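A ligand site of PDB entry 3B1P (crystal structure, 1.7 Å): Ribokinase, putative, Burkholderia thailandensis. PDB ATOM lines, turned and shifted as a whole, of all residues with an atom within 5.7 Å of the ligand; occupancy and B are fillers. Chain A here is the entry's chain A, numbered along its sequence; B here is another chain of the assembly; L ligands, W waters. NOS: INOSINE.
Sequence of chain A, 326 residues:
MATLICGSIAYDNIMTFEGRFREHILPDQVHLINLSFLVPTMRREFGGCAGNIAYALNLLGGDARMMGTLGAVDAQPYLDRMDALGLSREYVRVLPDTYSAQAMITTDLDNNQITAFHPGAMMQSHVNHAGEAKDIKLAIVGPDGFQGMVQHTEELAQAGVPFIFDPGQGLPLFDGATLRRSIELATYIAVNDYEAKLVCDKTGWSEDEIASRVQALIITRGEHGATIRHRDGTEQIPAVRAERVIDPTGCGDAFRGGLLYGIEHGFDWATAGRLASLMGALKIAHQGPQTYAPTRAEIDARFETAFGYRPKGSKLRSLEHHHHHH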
ATOM      1  N   SER A   8      12.683  -3.809  -1.080  1.00  0.00           N
ATOM      2  CA  SER A   8      12.786  -2.589  -0.297  1.00  0.00           C
ATOM      3  C   SER A   8      14.242  -2.101  -0.211  1.00  0.00           C
ATOM      4  O   SER A   8      15.221  -2.882  -0.302  1.00  0.00           O
ATOM      5  CB  SER A   8      12.233  -2.789   1.116  1.00  0.00           C
ATOM      6  OG  SER A   8      12.910  -3.826   1.777  1.00  0.00           O
ATOM      7  N   ALA A  10      16.070   0.568   2.439  1.00  0.00           N
ATOM      8  CA  ALA A  10      15.602   1.082   3.715  1.00  0.00           C
ATOM      9  C   ALA A  10      16.718   1.327   4.704  1.00  0.00           C
ATOM     10  O   ALA A  10      17.848   0.766   4.588  1.00  0.00           O
ATOM     11  CB  ALA A  10      14.543   0.117   4.303  1.00  0.00           C
ATOM     12  N   TYR A  11      16.451   2.186   5.695  1.00  0.00           N
ATOM     13  CA  TYR A  11      17.377   2.358   6.767  1.00  0.00           C
ATOM     14  C   TYR A  11      16.895   1.577   7.978  1.00  0.00           C
ATOM     15  O   TYR A  11      15.707   1.703   8.375  1.00  0.00           O
ATOM     16  CB  TYR A  11      17.534   3.858   7.152  1.00  0.00           C
ATOM     17  CG  TYR A  11      18.122   4.710   6.059  1.00  0.00           C
ATOM     18  CD1 TYR A  11      19.447   4.524   5.637  1.00  0.00           C
ATOM     19  CD2 TYR A  11      17.359   5.701   5.442  1.00  0.00           C
ATOM     20  CE1 TYR A  11      20.016   5.323   4.628  1.00  0.00           C
ATOM     21  CE2 TYR A  11      17.883   6.514   4.417  1.00  0.00           C
ATOM     22  CZ  TYR A  11      19.229   6.313   4.010  1.00  0.00           C
ATOM     23  OH  TYR A  11      19.736   7.126   3.001  1.00  0.00           O
ATOM     24  N   ASP A  12      17.790   0.805   8.587  1.00  0.00           N
ATOM     25  CA  ASP A  12      17.396  -0.113   9.667  1.00  0.00           C
ATOM     26  C   ASP A  12      17.895   0.356  11.013  1.00  0.00           C
ATOM     27  O   ASP A  12      19.056   0.819  11.111  1.00  0.00           O
ATOM     28  CB  ASP A  12      17.990  -1.563   9.468  1.00  0.00           C
ATOM     29  CG  ASP A  12      17.364  -2.298   8.344  1.00  0.00           C
ATOM     30  OD1 ASP A  12      16.316  -1.920   7.814  1.00  0.00           O
ATOM     31  OD2 ASP A  12      17.929  -3.339   7.949  1.00  0.00           O
ATOM     32  N   PHE A  46      22.414   0.484   6.808  1.00  0.00           N
ATOM     33  CA  PHE A  46      21.922   0.344   5.482  1.00  0.00           C
ATOM     34  C   PHE A  46      21.252  -1.014   5.359  1.00  0.00           C
ATOM     35  O   PHE A  46      21.866  -2.040   5.680  1.00  0.00           O
ATOM     36  CB  PHE A  46      23.079   0.458   4.485  1.00  0.00           C
ATOM     37  CG  PHE A  46      23.697   1.830   4.467  1.00  0.00           C
ATOM     38  CD1 PHE A  46      24.924   2.073   5.066  1.00  0.00           C
ATOM     39  CD2 PHE A  46      23.041   2.859   3.810  1.00  0.00           C
ATOM     40  CE1 PHE A  46      25.516   3.374   5.029  1.00  0.00           C
ATOM     41  CE2 PHE A  46      23.596   4.153   3.776  1.00  0.00           C
ATOM     42  CZ  PHE A  46      24.844   4.398   4.367  1.00  0.00           C
ATOM     43  N   GLY A  47      19.995  -0.971   4.934  1.00  0.00           N
ATOM     44  CA  GLY A  47      19.174  -2.182   4.814  1.00  0.00           C
ATOM     45  C   GLY A  47      18.172  -2.136   3.701  1.00  0.00           C
ATOM     46  O   GLY A  47      18.391  -1.547   2.651  1.00  0.00           O
ATOM     47  N   GLY A  48      17.034  -2.800   3.949  1.00  0.00           N
ATOM     48  CA  GLY A  48      16.066  -3.005   2.903  1.00  0.00           C
ATOM     49  C   GLY A  48      16.433  -4.344   2.215  1.00  0.00           C
ATOM     50  O   GLY A  48      17.663  -4.631   2.025  1.00  0.00           O
ATOM     51  N   CYS A  49      15.437  -5.092   1.724  1.00  0.00           N
ATOM     52  CA  CYS A  49      15.731  -6.473   1.288  1.00  0.00           C
ATOM     53  C   CYS A  49      16.510  -6.400   0.004  1.00  0.00           C
ATOM     54  O   CYS A  49      17.505  -7.121  -0.193  1.00  0.00           O
ATOM     55  CB  CYS A  49      14.465  -7.271   1.057  1.00  0.00           C
ATOM     56  SG  CYS A  49      13.555  -7.383   2.656  1.00  0.00           S
ATOM     57  N   ASN A  52      20.159  -5.386   0.760  1.00  0.00           N
ATOM     58  CA  ASN A  52      20.946  -6.475   1.374  1.00  0.00           C
ATOM     59  C   ASN A  52      21.277  -7.551   0.353  1.00  0.00           C
ATOM     60  O   ASN A  52      22.402  -8.063   0.363  1.00  0.00           O
ATOM     61  CB  ASN A  52      20.118  -7.135   2.520  1.00  0.00           C
ATOM     62  CG  ASN A  52      19.728  -6.136   3.642  1.00  0.00           C
ATOM     63  OD1 ASN A  52      20.344  -5.077   3.804  1.00  0.00           O
ATOM     64  ND2 ASN A  52      18.689  -6.523   4.433  1.00  0.00           N
ATOM     65  N   ALA A 103      13.043   0.804   9.120  1.00  0.00           N
ATOM     66  CA  ALA A 103      12.625  -0.374   9.895  1.00  0.00           C
ATOM     67  C   ALA A 103      13.199  -0.278  11.322  1.00  0.00           C
ATOM     68  O   ALA A 103      14.393  -0.015  11.516  1.00  0.00           O
ATOM     69  CB  ALA A 103      13.130  -1.645   9.217  1.00  0.00           C
ATOM     70  N   ILE A 105      13.728  -2.826  14.065  1.00  0.00           N
ATOM     71  CA  ILE A 105      13.696  -4.286  14.070  1.00  0.00           C
ATOM     72  C   ILE A 105      14.091  -4.729  15.456  1.00  0.00           C
ATOM     73  O   ILE A 105      15.175  -4.433  15.932  1.00  0.00           O
ATOM     74  CB  ILE A 105      14.737  -4.826  13.070  1.00  0.00           C
ATOM     75  CG1 ILE A 105      14.349  -4.356  11.669  1.00  0.00           C
ATOM     76  CG2 ILE A 105      14.754  -6.401  13.138  1.00  0.00           C
ATOM     77  CD1 ILE A 105      15.516  -4.623  10.639  1.00  0.00           C
ATOM     78  N   GLN A 113      12.216 -11.900  14.108  1.00  0.00           N
ATOM     79  CA  GLN A 113      12.192 -10.472  13.944  1.00  0.00           C
ATOM     80  C   GLN A 113      10.789 -10.000  14.121  1.00  0.00           C
ATOM     81  O   GLN A 113       9.871 -10.464  13.404  1.00  0.00           O
ATOM     82  CB  GLN A 113      12.709 -10.090  12.554  1.00  0.00           C
ATOM     83  CG  GLN A 113      14.128 -10.614  12.364  1.00  0.00           C
ATOM     84  CD  GLN A 113      14.965  -9.648  11.622  1.00  0.00           C
ATOM     85  OE1 GLN A 113      14.530  -9.074  10.593  1.00  0.00           O
ATOM     86  NE2 GLN A 113      16.170  -9.422  12.144  1.00  0.00           N
ATOM     87  N   THR A 115       9.206  -6.334  13.550  1.00  0.00           N
ATOM     88  CA  THR A 115       9.636  -5.059  12.957  1.00  0.00           C
ATOM     89  C   THR A 115       8.503  -4.071  12.856  1.00  0.00           C
ATOM     90  O   THR A 115       7.476  -4.386  12.233  1.00  0.00           O
ATOM     91  CB  THR A 115      10.133  -5.357  11.509  1.00  0.00           C
ATOM     92  OG1 THR A 115      11.305  -6.188  11.649  1.00  0.00           O
ATOM     93  CG2 THR A 115      10.567  -4.104  10.819  1.00  0.00           C
ATOM     94  N   PHE A 117       7.624  -1.056  10.838  1.00  0.00           N
ATOM     95  CA  PHE A 117       8.120  -0.565   9.513  1.00  0.00           C
ATOM     96  C   PHE A 117       7.374   0.686   9.076  1.00  0.00           C
ATOM     97  O   PHE A 117       6.139   0.702   8.997  1.00  0.00           O
ATOM     98  CB  PHE A 117       7.976  -1.691   8.515  1.00  0.00           C
ATOM     99  CG  PHE A 117       8.852  -1.538   7.276  1.00  0.00           C
ATOM    100  CD1 PHE A 117      10.201  -1.889   7.325  1.00  0.00           C
ATOM    101  CD2 PHE A 117       8.309  -1.054   6.080  1.00  0.00           C
ATOM    102  CE1 PHE A 117      11.016  -1.756   6.140  1.00  0.00           C
ATOM    103  CE2 PHE A 117       9.104  -0.922   4.903  1.00  0.00           C
ATOM    104  CZ  PHE A 117      10.446  -1.274   4.932  1.00  0.00           C
ATOM    105  N   MET A 122       8.744   3.374  -0.115  1.00  0.00           N
ATOM    106  CA  MET A 122       8.410   2.026  -0.519  1.00  0.00           C
ATOM    107  C   MET A 122       6.997   1.837  -0.990  1.00  0.00           C
ATOM    108  O   MET A 122       6.690   0.983  -1.818  1.00  0.00           O
ATOM    109  CB  MET A 122       8.769   1.024   0.626  1.00  0.00           C
ATOM    110  CG  MET A 122       8.650  -0.443   0.099  1.00  0.00           C
ATOM    111  SD  MET A 122       8.749  -1.640   1.456  1.00  0.00           S
ATOM    112  CE  MET A 122       6.993  -1.760   1.966  1.00  0.00           C
ATOM    113  N   PRO A 143      10.445  -8.514  -0.468  1.00  0.00           N
ATOM    114  CA  PRO A 143       9.463  -7.695   0.292  1.00  0.00           C
ATOM    115  C   PRO A 143       9.504  -6.224  -0.185  1.00  0.00           C
ATOM    116  O   PRO A 143      10.609  -5.601  -0.269  1.00  0.00           O
ATOM    117  CB  PRO A 143       9.967  -7.841   1.738  1.00  0.00           C
ATOM    118  CG  PRO A 143      10.572  -9.237   1.776  1.00  0.00           C
ATOM    119  CD  PRO A 143      11.377  -9.224   0.411  1.00  0.00           C
ATOM    120  N   ASP A 144       8.318  -5.677  -0.463  1.00  0.00           N
ATOM    121  CA  ASP A 144       8.275  -4.357  -1.092  1.00  0.00           C
ATOM    122  C   ASP A 144       6.894  -3.819  -0.874  1.00  0.00           C
ATOM    123  O   ASP A 144       6.047  -4.479  -0.200  1.00  0.00           O
ATOM    124  CB  ASP A 144       8.513  -4.515  -2.616  1.00  0.00           C
ATOM    125  CG  ASP A 144       9.275  -3.338  -3.216  1.00  0.00           C
ATOM    126  OD1 ASP A 144       9.214  -2.241  -2.655  1.00  0.00           O
ATOM    127  OD2 ASP A 144       9.952  -3.563  -4.222  1.00  0.00           O
ATOM    128  N   GLN A 169       8.680 -10.572   4.622  1.00  0.00           N
ATOM    129  CA  GLN A 169       7.869  -9.697   5.509  1.00  0.00           C
ATOM    130  C   GLN A 169       6.620  -9.128   4.837  1.00  0.00           C
ATOM    131  O   GLN A 169       5.689  -8.658   5.536  1.00  0.00           O
ATOM    132  CB  GLN A 169       8.707  -8.562   6.097  1.00  0.00           C
ATOM    133  CG  GLN A 169       9.862  -9.003   6.901  1.00  0.00           C
ATOM    134  CD  GLN A 169      11.160  -9.100   6.101  1.00  0.00           C
ATOM    135  OE1 GLN A 169      11.185  -9.491   4.913  1.00  0.00           O
ATOM    136  NE2 GLN A 169      12.247  -8.811   6.768  1.00  0.00           N
ATOM    137  N   GLY A 170       6.558  -9.175   3.500  1.00  0.00           N
ATOM    138  CA  GLY A 170       5.356  -8.780   2.758  1.00  0.00           C
ATOM    139  C   GLY A 170       4.220  -9.781   2.748  1.00  0.00           C
ATOM    140  O   GLY A 170       3.169  -9.525   2.205  1.00  0.00           O
ATOM    141  N   THR A 249      19.931 -10.402  11.609  1.00  0.00           N
ATOM    142  CA  THR A 249      19.136  -9.632  10.645  1.00  0.00           C
ATOM    143  C   THR A 249      19.769  -9.591   9.244  1.00  0.00           C
ATOM    144  O   THR A 249      20.913  -9.147   9.105  1.00  0.00           O
ATOM    145  CB  THR A 249      18.997  -8.162  11.116  1.00  0.00           C
ATOM    146  OG1 THR A 249      18.587  -8.180  12.467  1.00  0.00           O
ATOM    147  CG2 THR A 249      17.990  -7.453  10.253  1.00  0.00           C
ATOM    148  N   GLY A 250      19.009 -10.039   8.257  1.00  0.00           N
ATOM    149  CA  GLY A 250      19.452 -10.097   6.867  1.00  0.00           C
ATOM    150  C   GLY A 250      20.273 -11.333   6.541  1.00  0.00           C
ATOM    151  O   GLY A 250      20.833 -11.368   5.438  1.00  0.00           O
ATOM    152  N   ASP A 253      18.818 -12.649   3.472  1.00  0.00           N
ATOM    153  CA  ASP A 253      19.150 -11.821   2.260  1.00  0.00           C
ATOM    154  C   ASP A 253      20.561 -12.099   1.706  1.00  0.00           C
ATOM    155  O   ASP A 253      20.738 -12.143   0.464  1.00  0.00           O
ATOM    156  CB  ASP A 253      18.973 -10.346   2.574  1.00  0.00           C
ATOM    157  CG  ASP A 253      17.520  -9.975   2.807  1.00  0.00           C
ATOM    158  OD1 ASP A 253      16.628 -10.689   2.308  1.00  0.00           O
ATOM    159  OD2 ASP A 253      17.271  -8.954   3.494  1.00  0.00           O
ATOM    160  N   PRO A 289      22.759  -5.671   8.518  1.00  0.00           N
ATOM    161  CA  PRO A 289      22.714  -6.629   7.411  1.00  0.00           C
ATOM    162  C   PRO A 289      23.835  -6.541   6.376  1.00  0.00           C
ATOM    163  O   PRO A 289      24.003  -7.485   5.585  1.00  0.00           O
ATOM    164  CB  PRO A 289      21.366  -6.327   6.738  1.00  0.00           C
ATOM    165  CG  PRO A 289      21.070  -4.904   7.108  1.00  0.00           C
ATOM    166  CD  PRO A 289      21.668  -4.679   8.466  1.00  0.00           C
ATOM    167  N   SER B  36       6.153  -8.075  10.538  1.00  0.00           N
ATOM    168  CA  SER B  36       6.416  -6.676  10.241  1.00  0.00           C
ATOM    169  C   SER B  36       5.053  -5.987  10.167  1.00  0.00           C
ATOM    170  O   SER B  36       4.111  -6.526   9.623  1.00  0.00           O
ATOM    171  CB  SER B  36       7.197  -6.546   8.921  1.00  0.00           C
ATOM    172  OG  SER B  36       8.591  -6.757   9.157  1.00  0.00           O
ATOM    173  N   PHE B  37       4.951  -4.811  10.771  1.00  0.00           N
ATOM    174  CA  PHE B  37       3.689  -4.086  10.849  1.00  0.00           C
ATOM    175  C   PHE B  37       3.971  -2.625  10.627  1.00  0.00           C
ATOM    176  O   PHE B  37       5.031  -2.087  11.012  1.00  0.00           O
ATOM    177  CB  PHE B  37       2.938  -4.357  12.178  1.00  0.00           C
ATOM    178  CG  PHE B  37       3.693  -3.985  13.428  1.00  0.00           C
ATOM    179  CD1 PHE B  37       4.635  -4.849  13.994  1.00  0.00           C
ATOM    180  CD2 PHE B  37       3.448  -2.800  14.072  1.00  0.00           C
ATOM    181  CE1 PHE B  37       5.311  -4.458  15.185  1.00  0.00           C
ATOM    182  CE2 PHE B  37       4.117  -2.421  15.192  1.00  0.00           C
ATOM    183  CZ  PHE B  37       5.061  -3.262  15.766  1.00  0.00           C
ATOM    184  N   LEU B  38       3.009  -1.976   9.986  1.00  0.00           N
ATOM    185  CA  LEU B  38       3.195  -0.590   9.579  1.00  0.00           C
ATOM    186  C   LEU B  38       2.992   0.344  10.798  1.00  0.00           C
ATOM    187  O   LEU B  38       2.108   0.119  11.661  1.00  0.00           O
ATOM    188  CB  LEU B  38       2.420  -0.299   8.222  1.00  0.00           C
ATOM    189  CG  LEU B  38       2.819  -1.185   6.973  1.00  0.00           C
ATOM    190  CD1 LEU B  38       2.101  -0.894   5.616  1.00  0.00           C
ATOM    191  CD2 LEU B  38       4.373  -1.277   6.697  1.00  0.00           C
HETATM  192  N9  NOS L   1      12.171  -5.127   6.049  1.00  0.00           N
HETATM  193  C4  NOS L   1      11.176  -4.960   5.172  1.00  0.00           C
HETATM  194  N3  NOS L   1      11.065  -4.728   3.825  1.00  0.00           N
HETATM  195  C2  NOS L   1       9.890  -4.637   3.198  1.00  0.00           C
HETATM  196  N1  NOS L   1       8.729  -4.761   3.920  1.00  0.00           N
HETATM  197  C6  NOS L   1       8.724  -4.970   5.265  1.00  0.00           C
HETATM  198  O6  NOS L   1       7.542  -5.157   5.903  1.00  0.00           O
HETATM  199  C5  NOS L   1       9.969  -5.165   6.001  1.00  0.00           C
HETATM  200  N7  NOS L   1      10.332  -5.390   7.267  1.00  0.00           N
HETATM  201  C8  NOS L   1      11.714  -5.370   7.324  1.00  0.00           C
HETATM  202  C5' NOS L   1      15.842  -7.919   6.487  1.00  0.00           C
HETATM  203  O5' NOS L   1      15.521  -8.966   5.538  1.00  0.00           O
HETATM  204  C4' NOS L   1      15.363  -6.582   5.907  1.00  0.00           C
HETATM  205  O4' NOS L   1      13.942  -6.556   5.841  1.00  0.00           O
HETATM  206  C1' NOS L   1      13.591  -5.142   5.678  1.00  0.00           C
HETATM  207  C2' NOS L   1      14.520  -4.450   6.633  1.00  0.00           C
HETATM  208  O2' NOS L   1      14.847  -3.206   6.014  1.00  0.00           O
HETATM  209  C3' NOS L   1      15.728  -5.373   6.766  1.00  0.00           C
HETATM  210  O3' NOS L   1      16.934  -4.736   6.241  1.00  0.00           O
HETATM  211  O   HOH W   1       6.492  -5.399   2.442  1.00  0.00           O
HETATM  212  O   HOH W   2      12.719  -7.530   9.553  1.00  0.00           O
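The backbone NH (N) of Gly 48 is in hydrogen-bond range of an oxygen (O3') of the ligand, at 3.0 Å.
The side-chain carboxylate (OD2) of Asp 12 lies within hydrogen-bond range of an oxygen (O3') of the ligand, at 2.4 Å.
OD2 of Asp 253 lies within hydrogen-bond range of O5' of the ligand (2.7 Å).
The side-chain amide nitrogen (ND2) of Asn 52 is in hydrogen-bond range of an oxygen (O3') of the ligand.
SG of Cys 49 sits at hydrogen-bond distance from O4' of the ligand, 3.3 Å away.
The side-chain hydroxyl (OG) of Ser 36 of chain B sits at hydrogen-bond distance from a nitrogen (N7) of the ligand (2.9 Å).
OG of Ser 8 sits at hydrogen-bond distance from N3 of the ligand (2.9 Å).
The side-chain amide nitrogen (NE2) of Gln 169 is in hydrogen-bond range of an oxygen (O4') of the ligand (3.0 Å).
The backbone NH (N) of Ala 103 is in hydrogen-bond range of the backbone carbonyl oxygen (O) of Tyr 11 (2.9 Å).
The backbone NH (N) of Ser 8 lies within hydrogen-bond range of the backbone carbonyl oxygen (O) of Pro 143.
O of Phe 37 of chain B lies within hydrogen-bond range of N of Phe 117 (2.8 Å).
The backbone carbonyl oxygen (O) of Ala 10 sits at hydrogen-bond distance from the backbone NH (N) of Gly 47 (2.8 Å).
O of Thr 115 sits at hydrogen-bond distance from N of Phe 37 of chain B (2.9 Å).
The side-chain amide nitrogen (ND2) of Asn 52 sits close to the backbone carbonyl oxygen (O) of Gly 48 (3.2 Å).
The side-chain carboxylate of Asp 253 lies within hydrogen-bond range of the side-chain amide nitrogen of Asn 52, at 3.0 Å.
The side-chain hydroxyl of Ser 8 sits at hydrogen-bond distance from the backbone NH of Cys 49, 2.8 Å away.
Merely in contact with the ligand: Ala 10 (3.7 Å), Gly 47 (3.7 Å), Ala 103 (3.96 Å), Ile 105 (3.95 Å), Thr 115 (3.8 Å), Phe 117 (3.4 Å), Met 122 (3.6 Å) and Pro 143 (3.5 Å).
Within 4 Å of the ligand: Ser 8, Ala 10, Asp 12, Gly 47, Gly 48, Cys 49, Asn 52, Ala 103, Ile 105, Thr 115, Phe 117, Met 122, Pro 143, Gln 169, Asp 253 and Ser 36 of chain B.
Along chain A the residues within 4 Å of the ligand span positions 8 to 253.
Water W1 bridges N1 of the ligand (2.8 Å) and O of Asp 144 (2.8 Å).
Water W2 lies within hydrogen-bond range of OE1 of Gln 113, OG1 of Thr 115 and NE2 of Gln 169.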
